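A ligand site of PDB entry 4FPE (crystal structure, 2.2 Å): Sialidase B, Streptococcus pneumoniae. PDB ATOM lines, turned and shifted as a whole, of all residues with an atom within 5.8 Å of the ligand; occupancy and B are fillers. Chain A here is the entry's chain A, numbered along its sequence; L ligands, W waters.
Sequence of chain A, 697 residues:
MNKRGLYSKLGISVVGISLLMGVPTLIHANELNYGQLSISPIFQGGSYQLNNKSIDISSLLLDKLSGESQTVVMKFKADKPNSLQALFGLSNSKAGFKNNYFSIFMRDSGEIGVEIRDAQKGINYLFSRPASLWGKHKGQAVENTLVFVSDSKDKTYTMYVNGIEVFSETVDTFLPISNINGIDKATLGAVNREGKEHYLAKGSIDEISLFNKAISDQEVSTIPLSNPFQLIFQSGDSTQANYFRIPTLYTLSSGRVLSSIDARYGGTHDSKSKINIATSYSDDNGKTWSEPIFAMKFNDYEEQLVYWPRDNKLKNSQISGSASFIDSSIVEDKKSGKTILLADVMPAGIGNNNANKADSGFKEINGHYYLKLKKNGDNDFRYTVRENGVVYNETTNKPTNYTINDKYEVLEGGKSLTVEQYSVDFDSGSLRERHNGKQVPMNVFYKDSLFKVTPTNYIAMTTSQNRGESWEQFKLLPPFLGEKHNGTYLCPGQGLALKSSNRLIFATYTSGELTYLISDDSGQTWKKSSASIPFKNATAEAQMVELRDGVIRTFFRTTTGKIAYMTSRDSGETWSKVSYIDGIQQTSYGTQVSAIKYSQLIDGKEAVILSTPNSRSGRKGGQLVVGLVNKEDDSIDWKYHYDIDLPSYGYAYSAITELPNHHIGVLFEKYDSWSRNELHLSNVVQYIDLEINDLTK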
ATOM      1  N   ARG A 245     -19.023 -16.282 -18.750  1.00  0.00           N
ATOM      2  CA  ARG A 245     -17.715 -16.604 -18.167  1.00  0.00           C
ATOM      3  C   ARG A 245     -17.910 -17.400 -16.881  1.00  0.00           C
ATOM      4  O   ARG A 245     -19.027 -17.466 -16.336  1.00  0.00           O
ATOM      5  CB  ARG A 245     -16.896 -15.322 -17.896  1.00  0.00           C
ATOM      6  CG  ARG A 245     -16.098 -14.802 -19.099  1.00  0.00           C
ATOM      7  CD  ARG A 245     -14.801 -14.059 -18.666  1.00  0.00           C
ATOM      8  NE  ARG A 245     -13.927 -14.950 -17.901  1.00  0.00           N
ATOM      9  CZ  ARG A 245     -12.843 -14.570 -17.235  1.00  0.00           C
ATOM     10  NH1 ARG A 245     -12.451 -13.284 -17.234  1.00  0.00           N
ATOM     11  NH2 ARG A 245     -12.130 -15.480 -16.577  1.00  0.00           N
ATOM     12  N   ILE A 246     -16.820 -17.965 -16.390  1.00  0.00           N
ATOM     13  CA  ILE A 246     -16.807 -18.627 -15.084  1.00  0.00           C
ATOM     14  C   ILE A 246     -17.763 -19.828 -14.994  1.00  0.00           C
ATOM     15  O   ILE A 246     -18.696 -19.816 -14.200  1.00  0.00           O
ATOM     16  CB  ILE A 246     -17.148 -17.637 -13.940  1.00  0.00           C
ATOM     17  CG1 ILE A 246     -16.569 -16.237 -14.234  1.00  0.00           C
ATOM     18  CG2 ILE A 246     -16.598 -18.139 -12.639  1.00  0.00           C
ATOM     19  CD1 ILE A 246     -15.039 -16.185 -14.296  1.00  0.00           C
ATOM     20  N   ARG A 264     -23.039 -12.741 -18.601  1.00  0.00           N
ATOM     21  CA  ARG A 264     -22.478 -11.396 -18.594  1.00  0.00           C
ATOM     22  C   ARG A 264     -23.033 -10.539 -19.719  1.00  0.00           C
ATOM     23  O   ARG A 264     -22.913 -10.881 -20.908  1.00  0.00           O
ATOM     24  CB  ARG A 264     -20.941 -11.432 -18.612  1.00  0.00           C
ATOM     25  CG  ARG A 264     -20.354 -12.247 -17.445  1.00  0.00           C
ATOM     26  CD  ARG A 264     -18.858 -12.050 -17.353  1.00  0.00           C
ATOM     27  NE  ARG A 264     -18.329 -12.504 -16.069  1.00  0.00           N
ATOM     28  CZ  ARG A 264     -17.090 -12.251 -15.629  1.00  0.00           C
ATOM     29  NH1 ARG A 264     -16.244 -11.543 -16.376  1.00  0.00           N
ATOM     30  NH2 ARG A 264     -16.708 -12.696 -14.450  1.00  0.00           N
ATOM     31  N   ASP A 270     -15.380  -8.220 -15.986  1.00  0.00           N
ATOM     32  CA  ASP A 270     -15.674  -8.602 -14.593  1.00  0.00           C
ATOM     33  C   ASP A 270     -16.522  -7.518 -13.922  1.00  0.00           C
ATOM     34  O   ASP A 270     -17.467  -7.807 -13.172  1.00  0.00           O
ATOM     35  CB  ASP A 270     -14.368  -8.678 -13.782  1.00  0.00           C
ATOM     36  CG  ASP A 270     -13.663 -10.023 -13.882  1.00  0.00           C
ATOM     37  OD1 ASP A 270     -14.080 -10.900 -14.674  1.00  0.00           O
ATOM     38  OD2 ASP A 270     -12.661 -10.200 -13.142  1.00  0.00           O
ATOM     39  N   SER A 271     -16.148  -6.281 -14.200  1.00  0.00           N
ATOM     40  CA  SER A 271     -16.605  -5.125 -13.435  1.00  0.00           C
ATOM     41  C   SER A 271     -15.963  -3.867 -14.017  1.00  0.00           C
ATOM     42  O   SER A 271     -14.766  -3.887 -14.337  1.00  0.00           O
ATOM     43  CB  SER A 271     -16.202  -5.257 -11.967  1.00  0.00           C
ATOM     44  OG  SER A 271     -16.919  -4.321 -11.182  1.00  0.00           O
ATOM     45  N   ILE A 326     -21.059 -12.295  -9.455  1.00  0.00           N
ATOM     46  CA  ILE A 326     -19.899 -12.766 -10.212  1.00  0.00           C
ATOM     47  C   ILE A 326     -19.309 -13.970  -9.470  1.00  0.00           C
ATOM     48  O   ILE A 326     -19.358 -13.989  -8.244  1.00  0.00           O
ATOM     49  CB  ILE A 326     -18.830 -11.644 -10.433  1.00  0.00           C
ATOM     50  CG1 ILE A 326     -17.674 -12.132 -11.288  1.00  0.00           C
ATOM     51  CG2 ILE A 326     -18.318 -11.068  -9.113  1.00  0.00           C
ATOM     52  CD1 ILE A 326     -16.660 -11.020 -11.602  1.00  0.00           C
ATOM     53  N   ASP A 327     -18.808 -14.970 -10.196  1.00  0.00           N
ATOM     54  CA  ASP A 327     -18.148 -16.142  -9.595  1.00  0.00           C
ATOM     55  C   ASP A 327     -19.106 -17.014  -8.764  1.00  0.00           C
ATOM     56  O   ASP A 327     -19.329 -16.740  -7.580  1.00  0.00           O
ATOM     57  CB  ASP A 327     -16.964 -15.728  -8.697  1.00  0.00           C
ATOM     58  CG  ASP A 327     -15.764 -15.201  -9.483  1.00  0.00           C
ATOM     59  OD1 ASP A 327     -15.746 -15.322 -10.727  1.00  0.00           O
ATOM     60  OD2 ASP A 327     -14.829 -14.661  -8.839  1.00  0.00           O
ATOM     61  N   ASP A 344     -20.457 -14.227  -5.507  1.00  0.00           N
ATOM     62  CA  ASP A 344     -20.174 -12.879  -5.019  1.00  0.00           C
ATOM     63  C   ASP A 344     -21.317 -11.961  -5.427  1.00  0.00           C
ATOM     64  O   ASP A 344     -21.929 -12.151  -6.486  1.00  0.00           O
ATOM     65  CB  ASP A 344     -18.867 -12.329  -5.599  1.00  0.00           C
ATOM     66  CG  ASP A 344     -17.645 -13.158  -5.216  1.00  0.00           C
ATOM     67  OD1 ASP A 344     -17.586 -13.654  -4.071  1.00  0.00           O
ATOM     68  OD2 ASP A 344     -16.730 -13.283  -6.059  1.00  0.00           O
ATOM     69  N   VAL A 345     -21.618 -10.966  -4.590  1.00  0.00           N
ATOM     70  CA  VAL A 345     -22.610  -9.953  -4.948  1.00  0.00           C
ATOM     71  C   VAL A 345     -21.974  -8.590  -4.853  1.00  0.00           C
ATOM     72  O   VAL A 345     -21.242  -8.304  -3.905  1.00  0.00           O
ATOM     73  CB  VAL A 345     -23.767  -9.858  -3.948  1.00  0.00           C
ATOM     74  CG1 VAL A 345     -25.041  -9.384  -4.659  1.00  0.00           C
ATOM     75  CG2 VAL A 345     -23.966 -11.162  -3.257  1.00  0.00           C
ATOM     76  N   MET A 346     -22.299  -7.734  -5.811  1.00  0.00           N
ATOM     77  CA  MET A 346     -21.820  -6.365  -5.808  1.00  0.00           C
ATOM     78  C   MET A 346     -22.984  -5.397  -6.021  1.00  0.00           C
ATOM     79  O   MET A 346     -23.791  -5.580  -6.939  1.00  0.00           O
ATOM     80  CB  MET A 346     -20.783  -6.156  -6.917  1.00  0.00           C
ATOM     81  CG  MET A 346     -19.564  -7.073  -6.793  1.00  0.00           C
ATOM     82  SD  MET A 346     -18.239  -6.598  -7.900  1.00  0.00           S
ATOM     83  CE  MET A 346     -18.877  -7.156  -9.487  1.00  0.00           C
ATOM     84  N   ASN A 457     -17.891  -5.907  -1.702  1.00  0.00           N
ATOM     85  CA  ASN A 457     -18.286  -7.216  -2.193  1.00  0.00           C
ATOM     86  C   ASN A 457     -18.819  -8.071  -1.046  1.00  0.00           C
ATOM     87  O   ASN A 457     -18.264  -8.061   0.057  1.00  0.00           O
ATOM     88  CB  ASN A 457     -17.093  -7.921  -2.857  1.00  0.00           C
ATOM     89  CG  ASN A 457     -15.927  -8.072  -1.894  1.00  0.00           C
ATOM     90  OD1 ASN A 457     -15.295  -7.090  -1.533  1.00  0.00           O
ATOM     91  ND2 ASN A 457     -15.663  -9.304  -1.457  1.00  0.00           N
ATOM     92  N   TYR A 458     -19.915  -8.786  -1.308  1.00  0.00           N
ATOM     93  CA  TYR A 458     -20.545  -9.686  -0.332  1.00  0.00           C
ATOM     94  C   TYR A 458     -20.525 -11.113  -0.900  1.00  0.00           C
ATOM     95  O   TYR A 458     -20.119 -11.312  -2.047  1.00  0.00           O
ATOM     96  CB  TYR A 458     -21.992  -9.243  -0.081  1.00  0.00           C
ATOM     97  CG  TYR A 458     -22.111  -7.808   0.421  1.00  0.00           C
ATOM     98  CD1 TYR A 458     -22.174  -7.535   1.781  1.00  0.00           C
ATOM     99  CD2 TYR A 458     -22.147  -6.739  -0.482  1.00  0.00           C
ATOM    100  CE1 TYR A 458     -22.272  -6.223   2.242  1.00  0.00           C
ATOM    101  CE2 TYR A 458     -22.241  -5.418  -0.031  1.00  0.00           C
ATOM    102  CZ  TYR A 458     -22.309  -5.168   1.337  1.00  0.00           C
ATOM    103  OH  TYR A 458     -22.395  -3.866   1.814  1.00  0.00           O
ATOM    104  N   TYR A 489     -13.425 -13.550  -1.177  1.00  0.00           N
ATOM    105  CA  TYR A 489     -13.881 -13.779  -2.551  1.00  0.00           C
ATOM    106  C   TYR A 489     -14.144 -15.266  -2.797  1.00  0.00           C
ATOM    107  O   TYR A 489     -13.260 -16.100  -2.574  1.00  0.00           O
ATOM    108  CB  TYR A 489     -12.849 -13.274  -3.548  1.00  0.00           C
ATOM    109  CG  TYR A 489     -12.674 -11.776  -3.540  1.00  0.00           C
ATOM    110  CD1 TYR A 489     -13.540 -10.958  -4.257  1.00  0.00           C
ATOM    111  CD2 TYR A 489     -11.630 -11.184  -2.843  1.00  0.00           C
ATOM    112  CE1 TYR A 489     -13.379  -9.587  -4.259  1.00  0.00           C
ATOM    113  CE2 TYR A 489     -11.459  -9.808  -2.836  1.00  0.00           C
ATOM    114  CZ  TYR A 489     -12.337  -9.020  -3.545  1.00  0.00           C
ATOM    115  OH  TYR A 489     -12.192  -7.648  -3.553  1.00  0.00           O
ATOM    116  N   TYR A 509     -11.109 -16.830  -0.997  1.00  0.00           N
ATOM    117  CA  TYR A 509      -9.793 -16.252  -0.802  1.00  0.00           C
ATOM    118  C   TYR A 509      -9.844 -14.779  -0.397  1.00  0.00           C
ATOM    119  O   TYR A 509     -10.852 -14.090  -0.602  1.00  0.00           O
ATOM    120  CB  TYR A 509      -8.907 -16.410  -2.044  1.00  0.00           C
ATOM    121  CG  TYR A 509      -9.395 -15.669  -3.285  1.00  0.00           C
ATOM    122  CD1 TYR A 509      -8.914 -14.400  -3.598  1.00  0.00           C
ATOM    123  CD2 TYR A 509     -10.308 -16.249  -4.144  1.00  0.00           C
ATOM    124  CE1 TYR A 509      -9.341 -13.724  -4.731  1.00  0.00           C
ATOM    125  CE2 TYR A 509     -10.745 -15.592  -5.289  1.00  0.00           C
ATOM    126  CZ  TYR A 509     -10.263 -14.336  -5.573  1.00  0.00           C
ATOM    127  OH  TYR A 509     -10.714 -13.680  -6.713  1.00  0.00           O
ATOM    128  N   THR A 539      -5.104 -13.637  -6.544  1.00  0.00           N
ATOM    129  CA  THR A 539      -6.388 -14.204  -6.915  1.00  0.00           C
ATOM    130  C   THR A 539      -6.255 -15.709  -6.737  1.00  0.00           C
ATOM    131  O   THR A 539      -6.068 -16.449  -7.694  1.00  0.00           O
ATOM    132  CB  THR A 539      -6.726 -13.856  -8.391  1.00  0.00           C
ATOM    133  OG1 THR A 539      -6.585 -12.438  -8.568  1.00  0.00           O
ATOM    134  CG2 THR A 539      -8.156 -14.279  -8.746  1.00  0.00           C
ATOM    135  N   GLU A 541      -7.756 -18.510  -6.486  1.00  0.00           N
ATOM    136  CA  GLU A 541      -8.887 -19.387  -6.760  1.00  0.00           C
ATOM    137  C   GLU A 541      -8.491 -20.832  -6.475  1.00  0.00           C
ATOM    138  O   GLU A 541      -7.511 -21.334  -7.039  1.00  0.00           O
ATOM    139  CB  GLU A 541      -9.376 -19.197  -8.213  1.00  0.00           C
ATOM    140  CG  GLU A 541     -10.016 -17.816  -8.430  1.00  0.00           C
ATOM    141  CD  GLU A 541      -9.936 -17.327  -9.870  1.00  0.00           C
ATOM    142  OE1 GLU A 541     -10.752 -16.446 -10.240  1.00  0.00           O
ATOM    143  OE2 GLU A 541      -9.053 -17.806 -10.624  1.00  0.00           O
ATOM    144  N   ARG A 557      -4.703 -21.259  -7.627  1.00  0.00           N
ATOM    145  CA  ARG A 557      -4.011 -20.297  -8.481  1.00  0.00           C
ATOM    146  C   ARG A 557      -3.099 -19.397  -7.645  1.00  0.00           C
ATOM    147  O   ARG A 557      -3.458 -18.995  -6.546  1.00  0.00           O
ATOM    148  CB  ARG A 557      -5.082 -19.444  -9.166  1.00  0.00           C
ATOM    149  CG  ARG A 557      -4.577 -18.266  -9.957  1.00  0.00           C
ATOM    150  CD  ARG A 557      -5.775 -17.565 -10.583  1.00  0.00           C
ATOM    151  NE  ARG A 557      -5.388 -16.297 -11.186  1.00  0.00           N
ATOM    152  CZ  ARG A 557      -6.230 -15.544 -11.902  1.00  0.00           C
ATOM    153  NH1 ARG A 557      -7.488 -15.942 -12.110  1.00  0.00           N
ATOM    154  NH2 ARG A 557      -5.794 -14.402 -12.417  1.00  0.00           N
ATOM    155  N   GLY A 590      -1.799 -16.095 -13.524  1.00  0.00           N
ATOM    156  CA  GLY A 590      -2.434 -17.368 -13.210  1.00  0.00           C
ATOM    157  C   GLY A 590      -3.837 -17.527 -13.786  1.00  0.00           C
ATOM    158  O   GLY A 590      -4.417 -16.567 -14.303  1.00  0.00           O
ATOM    159  N   ARG A 619      -3.395 -17.775 -21.696  1.00  0.00           N
ATOM    160  CA  ARG A 619      -4.393 -18.790 -21.368  1.00  0.00           C
ATOM    161  C   ARG A 619      -4.676 -19.624 -22.601  1.00  0.00           C
ATOM    162  O   ARG A 619      -5.607 -19.351 -23.364  1.00  0.00           O
ATOM    163  CB  ARG A 619      -5.659 -18.132 -20.788  1.00  0.00           C
ATOM    164  CG  ARG A 619      -5.385 -17.352 -19.488  1.00  0.00           C
ATOM    165  CD  ARG A 619      -6.641 -16.825 -18.830  1.00  0.00           C
ATOM    166  NE  ARG A 619      -6.409 -16.459 -17.430  1.00  0.00           N
ATOM    167  CZ  ARG A 619      -7.240 -15.710 -16.701  1.00  0.00           C
ATOM    168  NH1 ARG A 619      -8.351 -15.228 -17.246  1.00  0.00           N
ATOM    169  NH2 ARG A 619      -6.949 -15.414 -15.437  1.00  0.00           N
ATOM    170  N   TYR A 653     -10.640 -20.379 -17.788  1.00  0.00           N
ATOM    171  CA  TYR A 653     -11.378 -20.951 -16.665  1.00  0.00           C
ATOM    172  C   TYR A 653     -12.060 -22.241 -17.103  1.00  0.00           C
ATOM    173  O   TYR A 653     -12.461 -22.379 -18.274  1.00  0.00           O
ATOM    174  CB  TYR A 653     -12.428 -19.978 -16.148  1.00  0.00           C
ATOM    175  CG  TYR A 653     -11.884 -18.931 -15.201  1.00  0.00           C
ATOM    176  CD1 TYR A 653     -10.753 -18.187 -15.524  1.00  0.00           C
ATOM    177  CD2 TYR A 653     -12.510 -18.680 -13.992  1.00  0.00           C
ATOM    178  CE1 TYR A 653     -10.263 -17.207 -14.669  1.00  0.00           C
ATOM    179  CE2 TYR A 653     -12.031 -17.689 -13.122  1.00  0.00           C
ATOM    180  CZ  TYR A 653     -10.913 -16.962 -13.466  1.00  0.00           C
ATOM    181  OH  TYR A 653     -10.434 -15.985 -12.598  1.00  0.00           O
ATOM    182  N   SER A 673      -9.188 -15.507 -21.883  1.00  0.00           N
ATOM    183  CA  SER A 673     -10.039 -14.530 -21.179  1.00  0.00           C
ATOM    184  C   SER A 673      -9.225 -13.496 -20.395  1.00  0.00           C
ATOM    185  O   SER A 673      -9.782 -12.690 -19.627  1.00  0.00           O
ATOM    186  CB  SER A 673     -11.037 -15.258 -20.267  1.00  0.00           C
ATOM    187  OG  SER A 673     -10.363 -16.003 -19.259  1.00  0.00           O
ATOM    188  N   TRP A 674      -7.905 -13.513 -20.559  1.00  0.00           N
ATOM    189  CA  TRP A 674      -7.068 -12.436 -20.005  1.00  0.00           C
ATOM    190  C   TRP A 674      -6.787 -11.413 -21.091  1.00  0.00           C
ATOM    191  O   TRP A 674      -6.818 -10.198 -20.848  1.00  0.00           O
ATOM    192  CB  TRP A 674      -5.735 -12.998 -19.486  1.00  0.00           C
ATOM    193  CG  TRP A 674      -4.907 -11.994 -18.733  1.00  0.00           C
ATOM    194  CD1 TRP A 674      -3.877 -11.235 -19.236  1.00  0.00           C
ATOM    195  CD2 TRP A 674      -5.019 -11.644 -17.355  1.00  0.00           C
ATOM    196  NE1 TRP A 674      -3.359 -10.440 -18.245  1.00  0.00           N
ATOM    197  CE2 TRP A 674      -4.041 -10.671 -17.072  1.00  0.00           C
ATOM    198  CE3 TRP A 674      -5.870 -12.069 -16.309  1.00  0.00           C
ATOM    199  CZ2 TRP A 674      -3.881 -10.105 -15.803  1.00  0.00           C
ATOM    200  CZ3 TRP A 674      -5.710 -11.518 -15.042  1.00  0.00           C
ATOM    201  CH2 TRP A 674      -4.723 -10.544 -14.805  1.00  0.00           C
HETATM  202  C1  LIG L   1     -16.809  -9.410  -6.290  1.00  0.00           C
HETATM  203  C2  LIG L   1     -13.736 -11.544  -8.226  1.00  0.00           C
HETATM  204  C3  LIG L   1     -13.297  -9.608  -9.635  1.00  0.00           C
HETATM  205  C4  LIG L   1     -14.796 -10.861  -7.615  1.00  0.00           C
HETATM  206  C5  LIG L   1     -14.354  -8.927  -9.014  1.00  0.00           C
HETATM  207  C6  LIG L   1     -10.874 -12.507 -11.895  1.00  0.00           C
HETATM  208  C7  LIG L   1     -11.848 -11.625  -9.895  1.00  0.00           C
HETATM  209  C8  LIG L   1     -11.044 -13.049 -13.326  1.00  0.00           C
HETATM  210  C9  LIG L   1     -12.990 -10.900  -9.232  1.00  0.00           C
HETATM  211  C10 LIG L   1     -15.100  -9.557  -8.006  1.00  0.00           C
HETATM  212  N1  LIG L   1     -12.146 -12.172 -11.207  1.00  0.00           N
HETATM  213  O1  LIG L   1      -9.373 -11.493 -14.564  1.00  0.00           O
HETATM  214  O2  LIG L   1      -8.472 -13.586 -13.765  1.00  0.00           O
HETATM  215  O3  LIG L   1      -9.948 -13.588 -15.674  1.00  0.00           O
HETATM  216  O4  LIG L   1     -16.153  -8.867  -7.396  1.00  0.00           O
HETATM  217  S1  LIG L   1      -9.625 -12.912 -14.366  1.00  0.00           S
HETATM  218  O   HOH W   1      -9.584 -10.622 -17.390  1.00  0.00           O
HETATM  219  O   HOH W   2     -13.463 -14.267 -11.791  1.00  0.00           O
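NH1 of Arg 619 lies within salt-bridge range of O3 of the ligand. The guanidinium group of Arg 245 lies within salt-bridge range of an oxygen (O3) of the ligand (3.0 Å). The guanidinium group (NH1) of Arg 557 lies within salt-bridge range of an oxygen (O2) of the ligand (3.0 Å). The side-chain carboxylate of Asp 270 lies within salt-bridge range of a nitrogen (N1) of the ligand, at 2.8 Å. OH of Tyr 653 sits close to O2 of the ligand, 3.3 Å away.
O of Ile 326 lies within hydrogen-bond range of N of Asp 344. The guanidinium group (NH1) of Arg 557 is in hydrogen-bond range of the side-chain hydroxyl (OH) of Tyr 653 (3.0 Å). NH2 of Arg 619 sits at hydrogen-bond distance from O of Gly 590 (3.0 Å). N of Tyr 489 is in hydrogen-bond range of O of Tyr 509, at 2.7 Å. OH of Tyr 653 is in hydrogen-bond range of OE1 of Glu 541. NH2 of Arg 245 lies within hydrogen-bond range of OG of Ser 673. OG of Ser 673 is in hydrogen-bond range of NH1 of Arg 619, 2.9 Å away. NH1 of Arg 245 is in salt-bridge range of OD1 of Asp 270, 3.9 Å away.
An oxygen (O4) of the ligand lies close to the side-chain sulfur of Met 346. Merely in contact with the ligand: Ile 326 (3.5 Å), Asp 327 (3.4 Å), Asp 344 (3.5 Å), Asn 457 (3.8 Å), Tyr 489 (3.6 Å), Tyr 509 (3.95 Å) and Trp 674 (3.7 Å). Hydrophobic or aromatic side chains that line the ligand: Ile 326, Met 346, Tyr 489, Tyr 653 and Trp 674. Of the 22 residues printed, 13 come within 4 Å of the ligand. The nearest printed residue that does not touch the ligand is Ser 673 (4.1 Å).
Water W2 bridges a nitrogen (N1) of the ligand and the side-chain carboxylate of Asp 327. Water W1 bridges an oxygen (O1) of the ligand (3.0 Å) and the backbone carbonyl oxygen of Ser 673 (3.1 Å).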
